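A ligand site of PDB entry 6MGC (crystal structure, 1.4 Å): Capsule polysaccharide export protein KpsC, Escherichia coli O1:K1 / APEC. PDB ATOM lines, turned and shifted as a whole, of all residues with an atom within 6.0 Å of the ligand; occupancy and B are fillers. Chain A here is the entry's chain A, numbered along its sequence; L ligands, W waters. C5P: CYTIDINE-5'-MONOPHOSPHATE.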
ATOM      1  N   PHE A  70       5.498  22.315 -18.837  1.00  0.00           N
ATOM      2  CA  PHE A  70       5.217  21.313 -19.856  1.00  0.00           C
ATOM      3  C   PHE A  70       6.120  20.083 -19.730  1.00  0.00           C
ATOM      4  O   PHE A  70       5.732  18.996 -20.201  1.00  0.00           O
ATOM      5  CB  PHE A  70       5.318  21.917 -21.255  1.00  0.00           C
ATOM      6  CG  PHE A  70       4.357  23.067 -21.478  1.00  0.00           C
ATOM      7  CD1 PHE A  70       3.002  22.891 -21.291  1.00  0.00           C
ATOM      8  CD2 PHE A  70       4.809  24.319 -21.852  1.00  0.00           C
ATOM      9  CE1 PHE A  70       2.098  23.935 -21.478  1.00  0.00           C
ATOM     10  CE2 PHE A  70       3.913  25.371 -22.026  1.00  0.00           C
ATOM     11  CZ  PHE A  70       2.556  25.165 -21.849  1.00  0.00           C
ATOM     12  N   SER A 133       8.223  13.852 -21.572  1.00  0.00           N
ATOM     13  CA  SER A 133       6.881  14.410 -21.578  1.00  0.00           C
ATOM     14  C   SER A 133       6.692  15.243 -20.304  1.00  0.00           C
ATOM     15  O   SER A 133       7.654  15.603 -19.618  1.00  0.00           O
ATOM     16  CB  SER A 133       5.842  13.286 -21.719  1.00  0.00           C
ATOM     17  OG  SER A 133       4.531  13.817 -21.841  1.00  0.00           O
ATOM     18  N   LYS A 134       5.443  15.565 -19.992  1.00  0.00           N
ATOM     19  CA  LYS A 134       5.162  16.318 -18.781  1.00  0.00           C
ATOM     20  C   LYS A 134       5.485  15.493 -17.552  1.00  0.00           C
ATOM     21  O   LYS A 134       6.095  15.985 -16.603  1.00  0.00           O
ATOM     22  CB  LYS A 134       3.691  16.736 -18.793  1.00  0.00           C
ATOM     23  CG  LYS A 134       3.326  17.712 -17.695  1.00  0.00           C
ATOM     24  CD  LYS A 134       1.879  18.126 -17.805  1.00  0.00           C
ATOM     25  CE  LYS A 134       1.510  19.120 -16.731  1.00  0.00           C
ATOM     26  NZ  LYS A 134       0.043  19.402 -16.757  1.00  0.00           N
ATOM     27  N   TYR A 135       5.115  14.205 -17.584  1.00  0.00           N
ATOM     28  CA  TYR A 135       5.456  13.214 -16.589  1.00  0.00           C
ATOM     29  C   TYR A 135       6.327  12.154 -17.270  1.00  0.00           C
ATOM     30  O   TYR A 135       6.268  11.999 -18.487  1.00  0.00           O
ATOM     31  CB  TYR A 135       4.167  12.586 -16.048  1.00  0.00           C
ATOM     32  CG  TYR A 135       3.089  13.609 -15.769  1.00  0.00           C
ATOM     33  CD1 TYR A 135       3.196  14.475 -14.680  1.00  0.00           C
ATOM     34  CD2 TYR A 135       1.965  13.732 -16.593  1.00  0.00           C
ATOM     35  CE1 TYR A 135       2.209  15.432 -14.427  1.00  0.00           C
ATOM     36  CE2 TYR A 135       0.990  14.683 -16.343  1.00  0.00           C
ATOM     37  CZ  TYR A 135       1.104  15.521 -15.263  1.00  0.00           C
ATOM     38  OH  TYR A 135       0.124  16.454 -15.029  1.00  0.00           O
ATOM     39  N   VAL A 154      -6.919   8.960 -30.357  1.00  0.00           N
ATOM     40  CA  VAL A 154      -7.915   9.877 -29.800  1.00  0.00           C
ATOM     41  C   VAL A 154      -7.573  10.030 -28.326  1.00  0.00           C
ATOM     42  O   VAL A 154      -7.522   9.029 -27.592  1.00  0.00           O
ATOM     43  CB  VAL A 154      -9.333   9.302 -29.962  1.00  0.00           C
ATOM     44  CG1 VAL A 154     -10.362  10.214 -29.290  1.00  0.00           C
ATOM     45  CG2 VAL A 154      -9.658   9.123 -31.446  1.00  0.00           C
ATOM     46  N   VAL A 155      -7.311  11.248 -27.889  1.00  0.00           N
ATOM     47  CA  VAL A 155      -6.721  11.501 -26.574  1.00  0.00           C
ATOM     48  C   VAL A 155      -7.799  11.882 -25.567  1.00  0.00           C
ATOM     49  O   VAL A 155      -8.463  12.915 -25.729  1.00  0.00           O
ATOM     50  CB  VAL A 155      -5.658  12.598 -26.686  1.00  0.00           C
ATOM     51  CG1 VAL A 155      -5.036  12.921 -25.329  1.00  0.00           C
ATOM     52  CG2 VAL A 155      -4.564  12.152 -27.683  1.00  0.00           C
ATOM     53  N   ASP A 156      -7.937  11.097 -24.499  1.00  0.00           N
ATOM     54  CA  ASP A 156      -8.843  11.487 -23.415  1.00  0.00           C
ATOM     55  C   ASP A 156      -8.122  12.390 -22.432  1.00  0.00           C
ATOM     56  O   ASP A 156      -6.882  12.464 -22.383  1.00  0.00           O
ATOM     57  CB  ASP A 156      -9.418  10.272 -22.674  1.00  0.00           C
ATOM     58  CG  ASP A 156     -10.797  10.538 -22.014  1.00  0.00           C
ATOM     59  OD1 ASP A 156     -11.277  11.682 -22.035  1.00  0.00           O
ATOM     60  OD2 ASP A 156     -11.378   9.531 -21.532  1.00  0.00           O
ATOM     61  N   GLN A 157      -8.915  13.095 -21.641  1.00  0.00           N
ATOM     62  CA  GLN A 157      -8.436  14.011 -20.630  1.00  0.00           C
ATOM     63  C   GLN A 157      -9.186  13.768 -19.329  1.00  0.00           C
ATOM     64  O   GLN A 157     -10.147  13.004 -19.283  1.00  0.00           O
ATOM     65  CB  GLN A 157      -8.602  15.463 -21.083  1.00  0.00           C
ATOM     66  CG  GLN A 157      -7.611  15.830 -22.177  1.00  0.00           C
ATOM     67  CD  GLN A 157      -7.854  17.196 -22.759  1.00  0.00           C
ATOM     68  OE1 GLN A 157      -8.280  17.329 -23.893  1.00  0.00           O
ATOM     69  NE2 GLN A 157      -7.509  18.218 -22.001  1.00  0.00           N
ATOM     70  N   THR A 158      -8.743  14.417 -18.267  1.00  0.00           N
ATOM     71  CA  THR A 158      -9.435  14.316 -16.986  1.00  0.00           C
ATOM     72  C   THR A 158     -10.706  15.161 -17.007  1.00  0.00           C
ATOM     73  O   THR A 158     -10.716  16.294 -17.489  1.00  0.00           O
ATOM     74  CB  THR A 158      -8.530  14.764 -15.836  1.00  0.00           C
ATOM     75  OG1 THR A 158      -8.130  16.121 -16.015  1.00  0.00           O
ATOM     76  CG2 THR A 158      -7.274  13.893 -15.749  1.00  0.00           C
ATOM     77  N   ASP A 161     -11.108  19.108 -16.493  1.00  0.00           N
ATOM     78  CA  ASP A 161      -9.817  19.770 -16.654  1.00  0.00           C
ATOM     79  C   ASP A 161     -10.051  21.237 -17.013  1.00  0.00           C
ATOM     80  O   ASP A 161     -10.793  21.531 -17.940  1.00  0.00           O
ATOM     81  CB  ASP A 161      -9.098  19.032 -17.821  1.00  0.00           C
ATOM     82  CG  ASP A 161      -7.672  19.546 -18.143  1.00  0.00           C
ATOM     83  OD1 ASP A 161      -7.218  20.575 -17.642  1.00  0.00           O
ATOM     84  OD2 ASP A 161      -7.024  18.849 -18.977  1.00  0.00           O
ATOM     85  N   SER A 163      -8.128  23.131 -18.619  1.00  0.00           N
ATOM     86  CA  SER A 163      -7.758  23.412 -20.012  1.00  0.00           C
ATOM     87  C   SER A 163      -8.882  23.111 -20.996  1.00  0.00           C
ATOM     88  O   SER A 163      -8.987  23.757 -22.043  1.00  0.00           O
ATOM     89  CB  SER A 163      -6.498  22.665 -20.475  1.00  0.00           C
ATOM     90  OG  SER A 163      -6.853  21.367 -20.943  1.00  0.00           O
ATOM     91  N   LYS A 193      -6.800   6.799 -25.865  1.00  0.00           N
ATOM     92  CA  LYS A 193      -5.765   6.758 -24.841  1.00  0.00           C
ATOM     93  C   LYS A 193      -6.284   7.388 -23.552  1.00  0.00           C
ATOM     94  O   LYS A 193      -6.632   8.572 -23.524  1.00  0.00           O
ATOM     95  CB  LYS A 193      -4.514   7.491 -25.335  1.00  0.00           C
ATOM     96  CG  LYS A 193      -3.380   7.586 -24.313  1.00  0.00           C
ATOM     97  CD  LYS A 193      -2.924   6.245 -23.830  1.00  0.00           C
ATOM     98  CE  LYS A 193      -1.702   6.376 -22.939  1.00  0.00           C
ATOM     99  NZ  LYS A 193      -1.998   7.233 -21.756  1.00  0.00           N
ATOM    100  N   VAL A 194      -6.325   6.589 -22.494  1.00  0.00           N
ATOM    101  CA  VAL A 194      -6.780   7.046 -21.191  1.00  0.00           C
ATOM    102  C   VAL A 194      -5.686   7.901 -20.540  1.00  0.00           C
ATOM    103  O   VAL A 194      -4.503   7.569 -20.621  1.00  0.00           O
ATOM    104  CB  VAL A 194      -7.127   5.852 -20.299  1.00  0.00           C
ATOM    105  CG1 VAL A 194      -7.569   6.329 -18.916  1.00  0.00           C
ATOM    106  CG2 VAL A 194      -8.202   5.002 -20.949  1.00  0.00           C
ATOM    107  N   HIS A 195      -6.097   8.982 -19.879  1.00  0.00           N
ATOM    108  CA  HIS A 195      -5.146   9.865 -19.200  1.00  0.00           C
ATOM    109  C   HIS A 195      -4.554   9.158 -17.979  1.00  0.00           C
ATOM    110  O   HIS A 195      -5.251   8.419 -17.287  1.00  0.00           O
ATOM    111  CB  HIS A 195      -5.896  11.120 -18.737  1.00  0.00           C
ATOM    112  CG  HIS A 195      -5.021  12.247 -18.290  1.00  0.00           C
ATOM    113  ND1 HIS A 195      -4.338  12.227 -17.091  1.00  0.00           N
ATOM    114  CD2 HIS A 195      -4.745  13.441 -18.852  1.00  0.00           C
ATOM    115  CE1 HIS A 195      -3.660  13.352 -16.951  1.00  0.00           C
ATOM    116  NE2 HIS A 195      -3.886  14.105 -18.019  1.00  0.00           N
ATOM    117  N   PRO A 196      -3.271   9.395 -17.668  1.00  0.00           N
ATOM    118  CA  PRO A 196      -2.651   8.708 -16.515  1.00  0.00           C
ATOM    119  C   PRO A 196      -3.268   9.026 -15.155  1.00  0.00           C
ATOM    120  O   PRO A 196      -3.273   8.148 -14.283  1.00  0.00           O
ATOM    121  CB  PRO A 196      -1.172   9.109 -16.593  1.00  0.00           C
ATOM    122  CG  PRO A 196      -1.157  10.346 -17.422  1.00  0.00           C
ATOM    123  CD  PRO A 196      -2.264  10.182 -18.415  1.00  0.00           C
ATOM    124  N   ASN A 222      -0.341   3.143 -18.963  1.00  0.00           N
ATOM    125  CA  ASN A 222       0.482   4.338 -18.786  1.00  0.00           C
ATOM    126  C   ASN A 222       1.755   4.142 -19.606  1.00  0.00           C
ATOM    127  O   ASN A 222       2.584   3.292 -19.278  1.00  0.00           O
ATOM    128  CB  ASN A 222       0.807   4.520 -17.312  1.00  0.00           C
ATOM    129  CG  ASN A 222       1.527   5.823 -17.020  1.00  0.00           C
ATOM    130  OD1 ASN A 222       1.363   6.814 -17.719  1.00  0.00           O
ATOM    131  ND2 ASN A 222       2.346   5.814 -15.973  1.00  0.00           N
ATOM    132  N   VAL A 223       1.887   4.909 -20.691  1.00  0.00           N
ATOM    133  CA  VAL A 223       3.031   4.780 -21.587  1.00  0.00           C
ATOM    134  C   VAL A 223       3.502   6.165 -22.013  1.00  0.00           C
ATOM    135  O   VAL A 223       2.728   7.128 -22.055  1.00  0.00           O
ATOM    136  CB  VAL A 223       2.734   3.904 -22.827  1.00  0.00           C
ATOM    137  CG1 VAL A 223       2.476   2.454 -22.392  1.00  0.00           C
ATOM    138  CG2 VAL A 223       1.569   4.464 -23.621  1.00  0.00           C
ATOM    139  N   PRO A 225       4.380   9.253 -24.202  1.00  0.00           N
ATOM    140  CA  PRO A 225       3.717   9.680 -25.458  1.00  0.00           C
ATOM    141  C   PRO A 225       4.552   9.504 -26.711  1.00  0.00           C
ATOM    142  O   PRO A 225       4.024   9.059 -27.733  1.00  0.00           O
ATOM    143  CB  PRO A 225       3.390  11.155 -25.178  1.00  0.00           C
ATOM    144  CG  PRO A 225       3.227  11.224 -23.692  1.00  0.00           C
ATOM    145  CD  PRO A 225       4.217  10.249 -23.129  1.00  0.00           C
ATOM    146  N   THR A 239      -8.060  19.540 -25.879  1.00  0.00           N
ATOM    147  CA  THR A 239      -7.081  20.548 -25.477  1.00  0.00           C
ATOM    148  C   THR A 239      -5.822  19.966 -24.864  1.00  0.00           C
ATOM    149  O   THR A 239      -4.971  20.738 -24.385  1.00  0.00           O
ATOM    150  CB  THR A 239      -7.691  21.562 -24.489  1.00  0.00           C
ATOM    151  OG1 THR A 239      -8.117  20.880 -23.308  1.00  0.00           O
ATOM    152  CG2 THR A 239      -8.858  22.350 -25.093  1.00  0.00           C
ATOM    153  N   SER A 240      -5.627  18.651 -24.884  1.00  0.00           N
ATOM    154  CA  SER A 240      -4.514  18.022 -24.183  1.00  0.00           C
ATOM    155  C   SER A 240      -3.150  18.516 -24.656  1.00  0.00           C
ATOM    156  O   SER A 240      -2.918  18.746 -25.847  1.00  0.00           O
ATOM    157  CB  SER A 240      -4.592  16.505 -24.401  1.00  0.00           C
ATOM    158  OG  SER A 240      -3.515  15.824 -23.768  1.00  0.00           O
ATOM    159  N   GLN A 241      -2.214  18.586 -23.716  1.00  0.00           N
ATOM    160  CA  GLN A 241      -0.817  18.779 -24.079  1.00  0.00           C
ATOM    161  C   GLN A 241      -0.354  17.737 -25.099  1.00  0.00           C
ATOM    162  O   GLN A 241       0.574  17.990 -25.879  1.00  0.00           O
ATOM    163  CB  GLN A 241       0.056  18.700 -22.815  1.00  0.00           C
ATOM    164  CG  GLN A 241       1.552  18.931 -23.023  1.00  0.00           C
ATOM    165  CD  GLN A 241       1.911  20.218 -23.728  1.00  0.00           C
ATOM    166  OE1 GLN A 241       1.109  21.144 -23.875  1.00  0.00           O
ATOM    167  NE2 GLN A 241       3.174  20.297 -24.152  1.00  0.00           N
ATOM    168  N   TYR A 242      -0.978  16.550 -25.116  1.00  0.00           N
ATOM    169  CA  TYR A 242      -0.644  15.524 -26.092  1.00  0.00           C
ATOM    170  C   TYR A 242      -0.631  16.070 -27.516  1.00  0.00           C
ATOM    171  O   TYR A 242       0.126  15.594 -28.368  1.00  0.00           O
ATOM    172  CB  TYR A 242      -1.675  14.383 -25.987  1.00  0.00           C
ATOM    173  CG  TYR A 242      -1.090  12.996 -25.999  1.00  0.00           C
ATOM    174  CD1 TYR A 242      -1.235  12.157 -24.907  1.00  0.00           C
ATOM    175  CD2 TYR A 242      -0.434  12.500 -27.126  1.00  0.00           C
ATOM    176  CE1 TYR A 242      -0.725  10.862 -24.928  1.00  0.00           C
ATOM    177  CE2 TYR A 242       0.080  11.228 -27.150  1.00  0.00           C
ATOM    178  CZ  TYR A 242      -0.070  10.408 -26.051  1.00  0.00           C
ATOM    179  OH  TYR A 242       0.445   9.133 -26.065  1.00  0.00           O
ATOM    180  N   GLU A 245       2.680  17.539 -28.263  1.00  0.00           N
ATOM    181  CA  GLU A 245       3.649  16.472 -28.340  1.00  0.00           C
ATOM    182  C   GLU A 245       3.540  15.716 -29.656  1.00  0.00           C
ATOM    183  O   GLU A 245       4.556  15.285 -30.213  1.00  0.00           O
ATOM    184  CB  GLU A 245       3.520  15.557 -27.136  1.00  0.00           C
ATOM    185  CG  GLU A 245       3.746  16.343 -25.848  1.00  0.00           C
ATOM    186  CD  GLU A 245       3.580  15.525 -24.611  1.00  0.00           C
ATOM    187  OE1 GLU A 245       4.589  15.150 -24.000  1.00  0.00           O
ATOM    188  OE2 GLU A 245       2.433  15.247 -24.248  1.00  0.00           O
HETATM  189  O3P C5P L   1      -4.094  16.027 -21.214  1.00  0.00           O
HETATM  190  P   C5P L   1      -3.051  16.781 -20.435  1.00  0.00           P
HETATM  191  O1P C5P L   1      -2.812  18.193 -20.934  1.00  0.00           O
HETATM  192  O2P C5P L   1      -3.258  16.740 -18.951  1.00  0.00           O
HETATM  193  O5' C5P L   1      -1.690  15.981 -20.699  1.00  0.00           O
HETATM  194  C5' C5P L   1      -0.567  16.057 -19.821  1.00  0.00           C
HETATM  195  C4' C5P L   1       0.324  14.863 -19.998  1.00  0.00           C
HETATM  196  O4' C5P L   1      -0.401  13.667 -19.622  1.00  0.00           O
HETATM  197  C3' C5P L   1       0.789  14.578 -21.414  1.00  0.00           C
HETATM  198  O3' C5P L   1       1.962  15.314 -21.723  1.00  0.00           O
HETATM  199  C2' C5P L   1       1.033  13.073 -21.414  1.00  0.00           C
HETATM  200  O2' C5P L   1       2.311  12.783 -20.875  1.00  0.00           O
HETATM  201  C1' C5P L   1      -0.019  12.595 -20.427  1.00  0.00           C
HETATM  202  N1  C5P L   1      -1.240  12.112 -21.085  1.00  0.00           N
HETATM  203  C2  C5P L   1      -1.271  10.722 -21.539  1.00  0.00           C
HETATM  204  N3  C5P L   1      -2.500  10.228 -22.170  1.00  0.00           N
HETATM  205  C4  C5P L   1      -3.616  11.125 -22.287  1.00  0.00           C
HETATM  206  C5  C5P L   1      -3.577  12.524 -21.821  1.00  0.00           C
HETATM  207  C6  C5P L   1      -2.349  13.021 -21.200  1.00  0.00           C
HETATM  208  O2  C5P L   1      -0.289  10.064 -21.430  1.00  0.00           O
HETATM  209  N4  C5P L   1      -4.808  10.601 -22.867  1.00  0.00           N
HETATM  210  O   HOH W   1       0.182   7.433 -19.937  1.00  0.00           O
HETATM  211  O   HOH W   2       2.655   9.719 -20.096  1.00  0.00           O
HETATM  212  O   HOH W   3      -1.333  19.734 -19.311  1.00  0.00           O
HETATM  213  O   HOH W   4       0.829   8.477 -23.435  1.00  0.00           O
HETATM  214  O   HOH W   5      -2.556  17.854 -16.687  1.00  0.00           O
HETATM  215  O   HOH W   6      -6.349  16.231 -18.987  1.00  0.00           O
HETATM  216  O   HOH W   7      -4.830  19.836 -20.431  1.00  0.00           O
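Residues that only touch the ligand: Lys 134 (3.7 Å), Tyr 135 (3.7 Å), Val 155 (3.4 Å), Gln 157 (3.7 Å), Val 194 (3.7 Å), Pro 196 (3.3 Å), Pro 225 (3.3 Å) and Tyr 242 (3.3 Å). Hydrophobic or aromatic side chains that line the ligand: Tyr 135, Val 155, His 195, Pro 196, Pro 225 and Tyr 242. Of the 23 residues printed, 15 come within 4 Å of the ligand. The nearest printed residue that does not touch the ligand is Val 223 (4.3 Å).
The side-chain hydroxyl (OG) of Ser 240 is in hydrogen-bond range of the backbone NH (N) of Tyr 242. OH of Tyr 135 sits at hydrogen-bond distance from NZ of Lys 134, at 3.4 Å. The backbone NH of Lys 134 sits close to the backbone carbonyl oxygen of Phe 70 (3.4 Å). NE2 of Gln 157 sits at hydrogen-bond distance from OG of Ser 163, 3.4 Å away. The backbone NH (N) of Ser 240 sits at hydrogen-bond distance from the side-chain amide oxygen (OE1) of Gln 157 (3.1 Å). N of Lys 193 sits at hydrogen-bond distance from O of Val 154, 2.9 Å away. N of Thr 239 sits at hydrogen-bond distance from OE1 of Gln 157 (3.0 Å). The backbone carbonyl oxygen (O) of Lys 193 lies within hydrogen-bond range of the backbone NH (N) of Asp 156.
The side-chain amino group (NZ) of Lys 193 lies within hydrogen-bond range of a nitrogen (N3) of the ligand, 3.1 Å away. O3P of the ligand is in hydrogen-bond range of OG of Ser 240, at 2.6 Å. The side-chain hydroxyl (OG) of Ser 133 is in hydrogen-bond range of an oxygen (O2') of the ligand (2.6 Å). The backbone carbonyl oxygen of Asp 156 is in hydrogen-bond range of a nitrogen (N4) of the ligand, 2.8 Å away. O1P of the ligand lies within hydrogen-bond range of N of Gln 241 (2.9 Å). O2P of the ligand is in hydrogen-bond range of NE2 of His 195, at 2.9 Å. N4 of the ligand sits at hydrogen-bond distance from O of Lys 193 (2.8 Å). The side-chain carboxylate (OE2) of Glu 245 lies within hydrogen-bond range of an oxygen (O3') of the ligand, 2.6 Å away.
Water W5 lies within hydrogen-bond range of O2P of the ligand (2.6 Å), NZ of Lys 134 (3.0 Å) and OH of Tyr 135 (3.4 Å). Water W7 lies within hydrogen-bond range of OG of Ser 163, O1P of the ligand and OD2 of Asp 161. Water W4 lies within hydrogen-bond range of the backbone carbonyl oxygen of Val 223 (2.7 Å), the side-chain hydroxyl of Tyr 242 (2.7 Å) and an oxygen (O2) of the ligand (2.8 Å). Water W1 lies within hydrogen-bond range of OD1 of Asn 222, NZ of Lys 193, O2 of the ligand and N of Val 223. Water W6 lies within hydrogen-bond range of the side-chain carboxylate (OD2) of Asp 161 (2.7 Å), the backbone NH (N) of Thr 158 (3.1 Å), an oxygen (O2P) of the ligand (3.1 Å) and a ring nitrogen (NE2) of His 195 (3.4 Å). Water W2 lies within hydrogen-bond range of an oxygen (O2') of the ligand (3.2 Å) and the backbone carbonyl oxygen (O) of Val 223 (3.2 Å).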
